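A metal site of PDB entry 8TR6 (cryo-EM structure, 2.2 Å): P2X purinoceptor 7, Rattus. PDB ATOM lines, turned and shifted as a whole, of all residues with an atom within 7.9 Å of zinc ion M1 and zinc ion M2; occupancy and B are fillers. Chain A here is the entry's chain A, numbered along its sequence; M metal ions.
Zinc ion M2 is bound by SG of Cys 479 (2.3 Å), SG of Cys 482 (2.3 Å), SG of Cys 498 (2.3 Å) and SG of Cys 477 (2.3 Å). Zinc ion M2 has four donor atoms within binding distance.
Four residues have an atom within 4 Å of zinc ion M1: Cys 479, Cys 499, Cys 506 and Cys 572. The nearest printed residue that does not touch zinc ion M1 is Ile 507 (4.2 Å).
Zinc ion M1 is bound by SG of Cys 572 (2.3 Å), SG of Cys 479 (2.3 Å), SG of Cys 506 (2.3 Å) and SG of Cys 499 (2.3 Å).
N of Gly 480 lies close to SG of Cys 477 (3.2 Å). NE2 of Gln 478 lies within hydrogen-bond range of O of Trp 476. SG of Cys 498 lies close to N of Gln 478. The side-chain sulfur (SG) of Cys 506 sits close to the side-chain hydroxyl (OG1) of Thr 508 (2.8 Å). The side-chain amide oxygen (OE1) of Gln 422 is in hydrogen-bond range of the backbone NH (N) of Cys 498 (2.5 Å). The side-chain sulfur (SG) of Cys 499 lies close to the backbone NH (N) of Ile 507 (3.7 Å). The side-chain amide oxygen of Asn 481 lies close to the backbone carbonyl oxygen of Cys 479 (3.3 Å). The backbone NH of Cys 572 lies close to the side-chain sulfur of Cys 482 (3.3 Å).
Merely in contact with zinc ion M2: Gln 478. Of the 28 residues printed, 5 come within 4 Å of zinc ion M2. The nearest printed residue that does not touch zinc ion M2 is Gly 480 (4.2 Å).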
ATOM      1  N   VAL A 404      23.263   9.615  -2.943  1.00  0.00           N
ATOM      2  CA  VAL A 404      22.653   9.877  -1.651  1.00  0.00           C
ATOM      3  C   VAL A 404      22.265   8.581  -0.963  1.00  0.00           C
ATOM      4  O   VAL A 404      22.288   8.485   0.271  1.00  0.00           O
ATOM      5  CB  VAL A 404      21.436  10.820  -1.824  1.00  0.00           C
ATOM      6  CG1 VAL A 404      20.212  10.039  -2.273  1.00  0.00           C
ATOM      7  CG2 VAL A 404      21.170  11.575  -0.542  1.00  0.00           C
ATOM      8  N   GLN A 422      26.548   6.306 -14.729  1.00  0.00           N
ATOM      9  CA  GLN A 422      25.781   5.642 -13.681  1.00  0.00           C
ATOM     10  C   GLN A 422      26.074   4.149 -13.632  1.00  0.00           C
ATOM     11  O   GLN A 422      26.171   3.560 -12.556  1.00  0.00           O
ATOM     12  CB  GLN A 422      24.279   5.874 -13.914  1.00  0.00           C
ATOM     13  CG  GLN A 422      23.412   5.470 -12.741  1.00  0.00           C
ATOM     14  CD  GLN A 422      23.142   6.607 -11.778  1.00  0.00           C
ATOM     15  OE1 GLN A 422      23.590   7.726 -11.989  1.00  0.00           O
ATOM     16  NE2 GLN A 422      22.396   6.319 -10.716  1.00  0.00           N
ATOM     17  N   SER A 473      11.602  10.463 -17.866  1.00  0.00           N
ATOM     18  CA  SER A 473      12.901  10.437 -17.199  1.00  0.00           C
ATOM     19  C   SER A 473      13.826   9.432 -17.879  1.00  0.00           C
ATOM     20  O   SER A 473      13.371   8.424 -18.424  1.00  0.00           O
ATOM     21  CB  SER A 473      12.724  10.079 -15.725  1.00  0.00           C
ATOM     22  OG  SER A 473      12.211   8.768 -15.584  1.00  0.00           O
ATOM     23  N   PRO A 474      15.137   9.683 -17.857  1.00  0.00           N
ATOM     24  CA  PRO A 474      16.070   8.721 -18.454  1.00  0.00           C
ATOM     25  C   PRO A 474      16.025   7.379 -17.738  1.00  0.00           C
ATOM     26  O   PRO A 474      15.709   7.296 -16.550  1.00  0.00           O
ATOM     27  CB  PRO A 474      17.439   9.395 -18.285  1.00  0.00           C
ATOM     28  CG  PRO A 474      17.151  10.835 -18.077  1.00  0.00           C
ATOM     29  CD  PRO A 474      15.830  10.890 -17.381  1.00  0.00           C
ATOM     30  N   TRP A 476      18.483   5.399 -16.905  1.00  0.00           N
ATOM     31  CA  TRP A 476      19.472   5.325 -15.836  1.00  0.00           C
ATOM     32  C   TRP A 476      19.074   6.141 -14.614  1.00  0.00           C
ATOM     33  O   TRP A 476      19.570   5.889 -13.517  1.00  0.00           O
ATOM     34  CB  TRP A 476      20.846   5.779 -16.340  1.00  0.00           C
ATOM     35  CG  TRP A 476      20.819   7.061 -17.111  1.00  0.00           C
ATOM     36  CD1 TRP A 476      20.838   7.211 -18.468  1.00  0.00           C
ATOM     37  CD2 TRP A 476      20.775   8.391 -16.573  1.00  0.00           C
ATOM     38  NE1 TRP A 476      20.810   8.547 -18.806  1.00  0.00           N
ATOM     39  CE2 TRP A 476      20.765   9.290 -17.659  1.00  0.00           C
ATOM     40  CE3 TRP A 476      20.738   8.913 -15.274  1.00  0.00           C
ATOM     41  CZ2 TRP A 476      20.727  10.670 -17.486  1.00  0.00           C
ATOM     42  CZ3 TRP A 476      20.693  10.280 -15.102  1.00  0.00           C
ATOM     43  CH2 TRP A 476      20.686  11.147 -16.206  1.00  0.00           C
ATOM     44  N   CYS A 477      18.186   7.122 -14.785  1.00  0.00           N
ATOM     45  CA  CYS A 477      17.764   7.954 -13.667  1.00  0.00           C
ATOM     46  C   CYS A 477      16.876   7.163 -12.709  1.00  0.00           C
ATOM     47  O   CYS A 477      16.185   6.221 -13.098  1.00  0.00           O
ATOM     48  CB  CYS A 477      17.019   9.188 -14.161  1.00  0.00           C
ATOM     49  SG  CYS A 477      16.255  10.156 -12.848  1.00  0.00           S
ATOM     50  N   GLN A 478      16.901   7.573 -11.438  1.00  0.00           N
ATOM     51  CA  GLN A 478      16.109   6.947 -10.392  1.00  0.00           C
ATOM     52  C   GLN A 478      15.471   7.982  -9.474  1.00  0.00           C
ATOM     53  O   GLN A 478      15.004   7.635  -8.383  1.00  0.00           O
ATOM     54  CB  GLN A 478      16.958   5.977  -9.558  1.00  0.00           C
ATOM     55  CG  GLN A 478      18.036   5.231 -10.348  1.00  0.00           C
ATOM     56  CD  GLN A 478      17.469   4.258 -11.348  1.00  0.00           C
ATOM     57  OE1 GLN A 478      16.387   3.697 -11.142  1.00  0.00           O
ATOM     58  NE2 GLN A 478      18.188   4.038 -12.446  1.00  0.00           N
ATOM     59  N   CYS A 479      15.434   9.249  -9.890  1.00  0.00           N
ATOM     60  CA  CYS A 479      14.874  10.318  -9.084  1.00  0.00           C
ATOM     61  C   CYS A 479      13.766  11.084  -9.786  1.00  0.00           C
ATOM     62  O   CYS A 479      13.019  11.807  -9.121  1.00  0.00           O
ATOM     63  CB  CYS A 479      15.967  11.301  -8.637  1.00  0.00           C
ATOM     64  SG  CYS A 479      16.512  12.457  -9.915  1.00  0.00           S
ATOM     65  N   GLY A 480      13.641  10.961 -11.106  1.00  0.00           N
ATOM     66  CA  GLY A 480      12.580  11.607 -11.837  1.00  0.00           C
ATOM     67  C   GLY A 480      12.839  13.056 -12.205  1.00  0.00           C
ATOM     68  O   GLY A 480      11.968  13.676 -12.823  1.00  0.00           O
ATOM     69  N   ASN A 481      13.999  13.607 -11.853  1.00  0.00           N
ATOM     70  CA  ASN A 481      14.328  14.988 -12.166  1.00  0.00           C
ATOM     71  C   ASN A 481      15.491  15.127 -13.135  1.00  0.00           C
ATOM     72  O   ASN A 481      15.736  16.231 -13.620  1.00  0.00           O
ATOM     73  CB  ASN A 481      14.655  15.764 -10.876  1.00  0.00           C
ATOM     74  CG  ASN A 481      13.476  15.856  -9.944  1.00  0.00           C
ATOM     75  OD1 ASN A 481      12.577  15.015  -9.966  1.00  0.00           O
ATOM     76  ND2 ASN A 481      13.464  16.879  -9.100  1.00  0.00           N
ATOM     77  N   CYS A 482      16.213  14.041 -13.428  1.00  0.00           N
ATOM     78  CA  CYS A 482      17.316  14.105 -14.368  1.00  0.00           C
ATOM     79  C   CYS A 482      16.797  14.265 -15.796  1.00  0.00           C
ATOM     80  O   CYS A 482      15.679  13.850 -16.120  1.00  0.00           O
ATOM     81  CB  CYS A 482      18.177  12.855 -14.271  1.00  0.00           C
ATOM     82  SG  CYS A 482      19.092  12.691 -12.712  1.00  0.00           S
ATOM     83  N   LEU A 483      17.614  14.881 -16.637  1.00  0.00           N
ATOM     84  CA  LEU A 483      17.289  15.141 -18.029  1.00  0.00           C
ATOM     85  C   LEU A 483      18.422  14.682 -18.916  1.00  0.00           C
ATOM     86  O   LEU A 483      19.574  14.590 -18.473  1.00  0.00           O
ATOM     87  CB  LEU A 483      17.023  16.629 -18.258  1.00  0.00           C
ATOM     88  CG  LEU A 483      15.996  17.276 -17.317  1.00  0.00           C
ATOM     89  CD1 LEU A 483      15.958  18.784 -17.535  1.00  0.00           C
ATOM     90  CD2 LEU A 483      14.623  16.665 -17.528  1.00  0.00           C
ATOM     91  N   LEU A 497      24.300  10.774 -15.198  1.00  0.00           N
ATOM     92  CA  LEU A 497      24.474  10.401 -13.800  1.00  0.00           C
ATOM     93  C   LEU A 497      23.299  10.923 -12.990  1.00  0.00           C
ATOM     94  O   LEU A 497      22.854  12.053 -13.183  1.00  0.00           O
ATOM     95  CB  LEU A 497      25.800  10.955 -13.252  1.00  0.00           C
ATOM     96  CG  LEU A 497      26.103  10.746 -11.767  1.00  0.00           C
ATOM     97  CD1 LEU A 497      26.516   9.310 -11.487  1.00  0.00           C
ATOM     98  CD2 LEU A 497      27.187  11.711 -11.329  1.00  0.00           C
ATOM     99  N   CYS A 498      22.809  10.097 -12.075  1.00  0.00           N
ATOM    100  CA  CYS A 498      21.703  10.437 -11.195  1.00  0.00           C
ATOM    101  C   CYS A 498      22.196  10.591  -9.766  1.00  0.00           C
ATOM    102  O   CYS A 498      23.263  10.099  -9.395  1.00  0.00           O
ATOM    103  CB  CYS A 498      20.599   9.374 -11.266  1.00  0.00           C
ATOM    104  SG  CYS A 498      19.128   9.743 -10.302  1.00  0.00           S
ATOM    105  N   CYS A 499      21.388  11.285  -8.961  1.00  0.00           N
ATOM    106  CA  CYS A 499      21.733  11.547  -7.565  1.00  0.00           C
ATOM    107  C   CYS A 499      21.650  10.299  -6.688  1.00  0.00           C
ATOM    108  O   CYS A 499      22.122  10.355  -5.548  1.00  0.00           O
ATOM    109  CB  CYS A 499      20.811  12.619  -6.998  1.00  0.00           C
ATOM    110  SG  CYS A 499      19.049  12.213  -7.041  1.00  0.00           S
ATOM    111  N   ARG A 500      21.074   9.207  -7.182  1.00  0.00           N
ATOM    112  CA  ARG A 500      20.914   8.016  -6.374  1.00  0.00           C
ATOM    113  C   ARG A 500      21.040   6.789  -7.259  1.00  0.00           C
ATOM    114  O   ARG A 500      20.873   6.848  -8.479  1.00  0.00           O
ATOM    115  CB  ARG A 500      19.559   8.005  -5.642  1.00  0.00           C
ATOM    116  CG  ARG A 500      18.376   8.385  -6.521  1.00  0.00           C
ATOM    117  CD  ARG A 500      17.088   8.486  -5.728  1.00  0.00           C
ATOM    118  NE  ARG A 500      17.097   7.634  -4.544  1.00  0.00           N
ATOM    119  CZ  ARG A 500      16.939   8.065  -3.295  1.00  0.00           C
ATOM    120  NH1 ARG A 500      16.750   9.339  -3.016  1.00  0.00           N
ATOM    121  NH2 ARG A 500      16.974   7.186  -2.300  1.00  0.00           N
ATOM    122  N   GLY A 504      13.927   6.698  -5.572  1.00  0.00           N
ATOM    123  CA  GLY A 504      13.623   7.414  -4.350  1.00  0.00           C
ATOM    124  C   GLY A 504      13.528   8.910  -4.624  1.00  0.00           C
ATOM    125  O   GLY A 504      13.511   9.341  -5.771  1.00  0.00           O
ATOM    126  N   GLN A 505      13.460   9.664  -3.540  1.00  0.00           N
ATOM    127  CA  GLN A 505      13.332  11.113  -3.648  1.00  0.00           C
ATOM    128  C   GLN A 505      14.633  11.741  -4.109  1.00  0.00           C
ATOM    129  O   GLN A 505      15.719  11.324  -3.708  1.00  0.00           O
ATOM    130  CB  GLN A 505      12.895  11.712  -2.308  1.00  0.00           C
ATOM    131  CG  GLN A 505      13.767  11.319  -1.130  1.00  0.00           C
ATOM    132  CD  GLN A 505      13.520  12.182   0.093  1.00  0.00           C
ATOM    133  OE1 GLN A 505      13.106  13.336  -0.027  1.00  0.00           O
ATOM    134  NE2 GLN A 505      13.754  11.621   1.269  1.00  0.00           N
ATOM    135  N   CYS A 506      14.513  12.759  -4.965  1.00  0.00           N
ATOM    136  CA  CYS A 506      15.686  13.453  -5.465  1.00  0.00           C
ATOM    137  C   CYS A 506      16.339  14.271  -4.356  1.00  0.00           C
ATOM    138  O   CYS A 506      15.665  14.819  -3.471  1.00  0.00           O
ATOM    139  CB  CYS A 506      15.312  14.364  -6.625  1.00  0.00           C
ATOM    140  SG  CYS A 506      16.713  15.226  -7.375  1.00  0.00           S
ATOM    141  N   ILE A 507      17.665  14.350  -4.403  1.00  0.00           N
ATOM    142  CA  ILE A 507      18.398  15.146  -3.420  1.00  0.00           C
ATOM    143  C   ILE A 507      18.052  16.620  -3.563  1.00  0.00           C
ATOM    144  O   ILE A 507      18.135  17.376  -2.588  1.00  0.00           O
ATOM    145  CB  ILE A 507      19.917  14.904  -3.581  1.00  0.00           C
ATOM    146  CG1 ILE A 507      20.671  15.539  -2.403  1.00  0.00           C
ATOM    147  CG2 ILE A 507      20.407  15.479  -4.895  1.00  0.00           C
ATOM    148  CD1 ILE A 507      22.152  15.315  -2.454  1.00  0.00           C
ATOM    149  N   THR A 508      17.661  17.043  -4.764  1.00  0.00           N
ATOM    150  CA  THR A 508      17.303  18.441  -4.965  1.00  0.00           C
ATOM    151  C   THR A 508      16.090  18.845  -4.132  1.00  0.00           C
ATOM    152  O   THR A 508      15.934  20.021  -3.787  1.00  0.00           O
ATOM    153  CB  THR A 508      17.034  18.712  -6.443  1.00  0.00           C
ATOM    154  OG1 THR A 508      15.941  17.899  -6.892  1.00  0.00           O
ATOM    155  CG2 THR A 508      18.263  18.423  -7.285  1.00  0.00           C
ATOM    156  N   THR A 509      15.222  17.881  -3.820  1.00  0.00           N
ATOM    157  CA  THR A 509      14.023  18.194  -3.048  1.00  0.00           C
ATOM    158  C   THR A 509      14.346  18.668  -1.635  1.00  0.00           C
ATOM    159  O   THR A 509      13.525  19.349  -1.023  1.00  0.00           O
ATOM    160  CB  THR A 509      13.108  16.972  -2.979  1.00  0.00           C
ATOM    161  OG1 THR A 509      13.819  15.868  -2.390  1.00  0.00           O
ATOM    162  CG2 THR A 509      12.648  16.578  -4.371  1.00  0.00           C
ATOM    163  N   PHE A 513      19.624  21.584  -0.053  1.00  0.00           N
ATOM    164  CA  PHE A 513      20.139  21.744  -1.401  1.00  0.00           C
ATOM    165  C   PHE A 513      19.927  23.164  -1.895  1.00  0.00           C
ATOM    166  O   PHE A 513      20.831  23.793  -2.459  1.00  0.00           O
ATOM    167  CB  PHE A 513      19.469  20.740  -2.345  1.00  0.00           C
ATOM    168  CG  PHE A 513      19.982  20.802  -3.754  1.00  0.00           C
ATOM    169  CD1 PHE A 513      19.452  21.701  -4.663  1.00  0.00           C
ATOM    170  CD2 PHE A 513      20.990  19.952  -4.178  1.00  0.00           C
ATOM    171  CE1 PHE A 513      19.920  21.745  -5.959  1.00  0.00           C
ATOM    172  CE2 PHE A 513      21.462  20.001  -5.466  1.00  0.00           C
ATOM    173  CZ  PHE A 513      20.923  20.903  -6.359  1.00  0.00           C
ATOM    174  N   TYR A 553      28.027  22.338  -4.354  1.00  0.00           N
ATOM    175  CA  TYR A 553      27.494  20.982  -4.303  1.00  0.00           C
ATOM    176  C   TYR A 553      28.628  19.963  -4.208  1.00  0.00           C
ATOM    177  O   TYR A 553      28.550  19.013  -3.424  1.00  0.00           O
ATOM    178  CB  TYR A 553      26.637  20.692  -5.531  1.00  0.00           C
ATOM    179  CG  TYR A 553      26.136  19.265  -5.588  1.00  0.00           C
ATOM    180  CD1 TYR A 553      26.911  18.256  -6.144  1.00  0.00           C
ATOM    181  CD2 TYR A 553      24.901  18.917  -5.055  1.00  0.00           C
ATOM    182  CE1 TYR A 553      26.456  16.955  -6.182  1.00  0.00           C
ATOM    183  CE2 TYR A 553      24.438  17.620  -5.091  1.00  0.00           C
ATOM    184  CZ  TYR A 553      25.226  16.638  -5.659  1.00  0.00           C
ATOM    185  OH  TYR A 553      24.779  15.349  -5.695  1.00  0.00           O
ATOM    186  N   PRO A 570      25.287  15.231 -10.456  1.00  0.00           N
ATOM    187  CA  PRO A 570      24.158  14.527 -11.069  1.00  0.00           C
ATOM    188  C   PRO A 570      23.443  15.414 -12.067  1.00  0.00           C
ATOM    189  O   PRO A 570      23.443  16.643 -11.962  1.00  0.00           O
ATOM    190  CB  PRO A 570      23.253  14.175  -9.875  1.00  0.00           C
ATOM    191  CG  PRO A 570      24.141  14.234  -8.696  1.00  0.00           C
ATOM    192  CD  PRO A 570      25.165  15.272  -8.989  1.00  0.00           C
ATOM    193  N   SER A 571      22.816  14.773 -13.063  1.00  0.00           N
ATOM    194  CA  SER A 571      22.117  15.526 -14.091  1.00  0.00           C
ATOM    195  C   SER A 571      20.996  16.372 -13.494  1.00  0.00           C
ATOM    196  O   SER A 571      20.797  17.524 -13.884  1.00  0.00           O
ATOM    197  CB  SER A 571      21.555  14.571 -15.146  1.00  0.00           C
ATOM    198  OG  SER A 571      20.765  15.269 -16.092  1.00  0.00           O
ATOM    199  N   CYS A 572      20.257  15.815 -12.534  1.00  0.00           N
ATOM    200  CA  CYS A 572      19.157  16.551 -11.923  1.00  0.00           C
ATOM    201  C   CYS A 572      19.655  17.829 -11.249  1.00  0.00           C
ATOM    202  O   CYS A 572      19.140  18.922 -11.501  1.00  0.00           O
ATOM    203  CB  CYS A 572      18.441  15.668 -10.901  1.00  0.00           C
ATOM    204  SG  CYS A 572      19.560  14.736  -9.827  1.00  0.00           S
ATOM    205  N   CYS A 573      20.661  17.693 -10.379  1.00  0.00           N
ATOM    206  CA  CYS A 573      21.190  18.855  -9.677  1.00  0.00           C
ATOM    207  C   CYS A 573      21.833  19.846 -10.648  1.00  0.00           C
ATOM    208  O   CYS A 573      21.644  21.062 -10.525  1.00  0.00           O
ATOM    209  CB  CYS A 573      22.199  18.399  -8.624  1.00  0.00           C
ATOM    210  SG  CYS A 573      21.669  16.945  -7.694  1.00  0.00           S
HETATM  211 ZN    ZN M   1      17.968  13.643  -8.536  1.00  0.00          ZN
HETATM  212 ZN    ZN M   2      17.767  11.251 -11.446  1.00  0.00          ZN
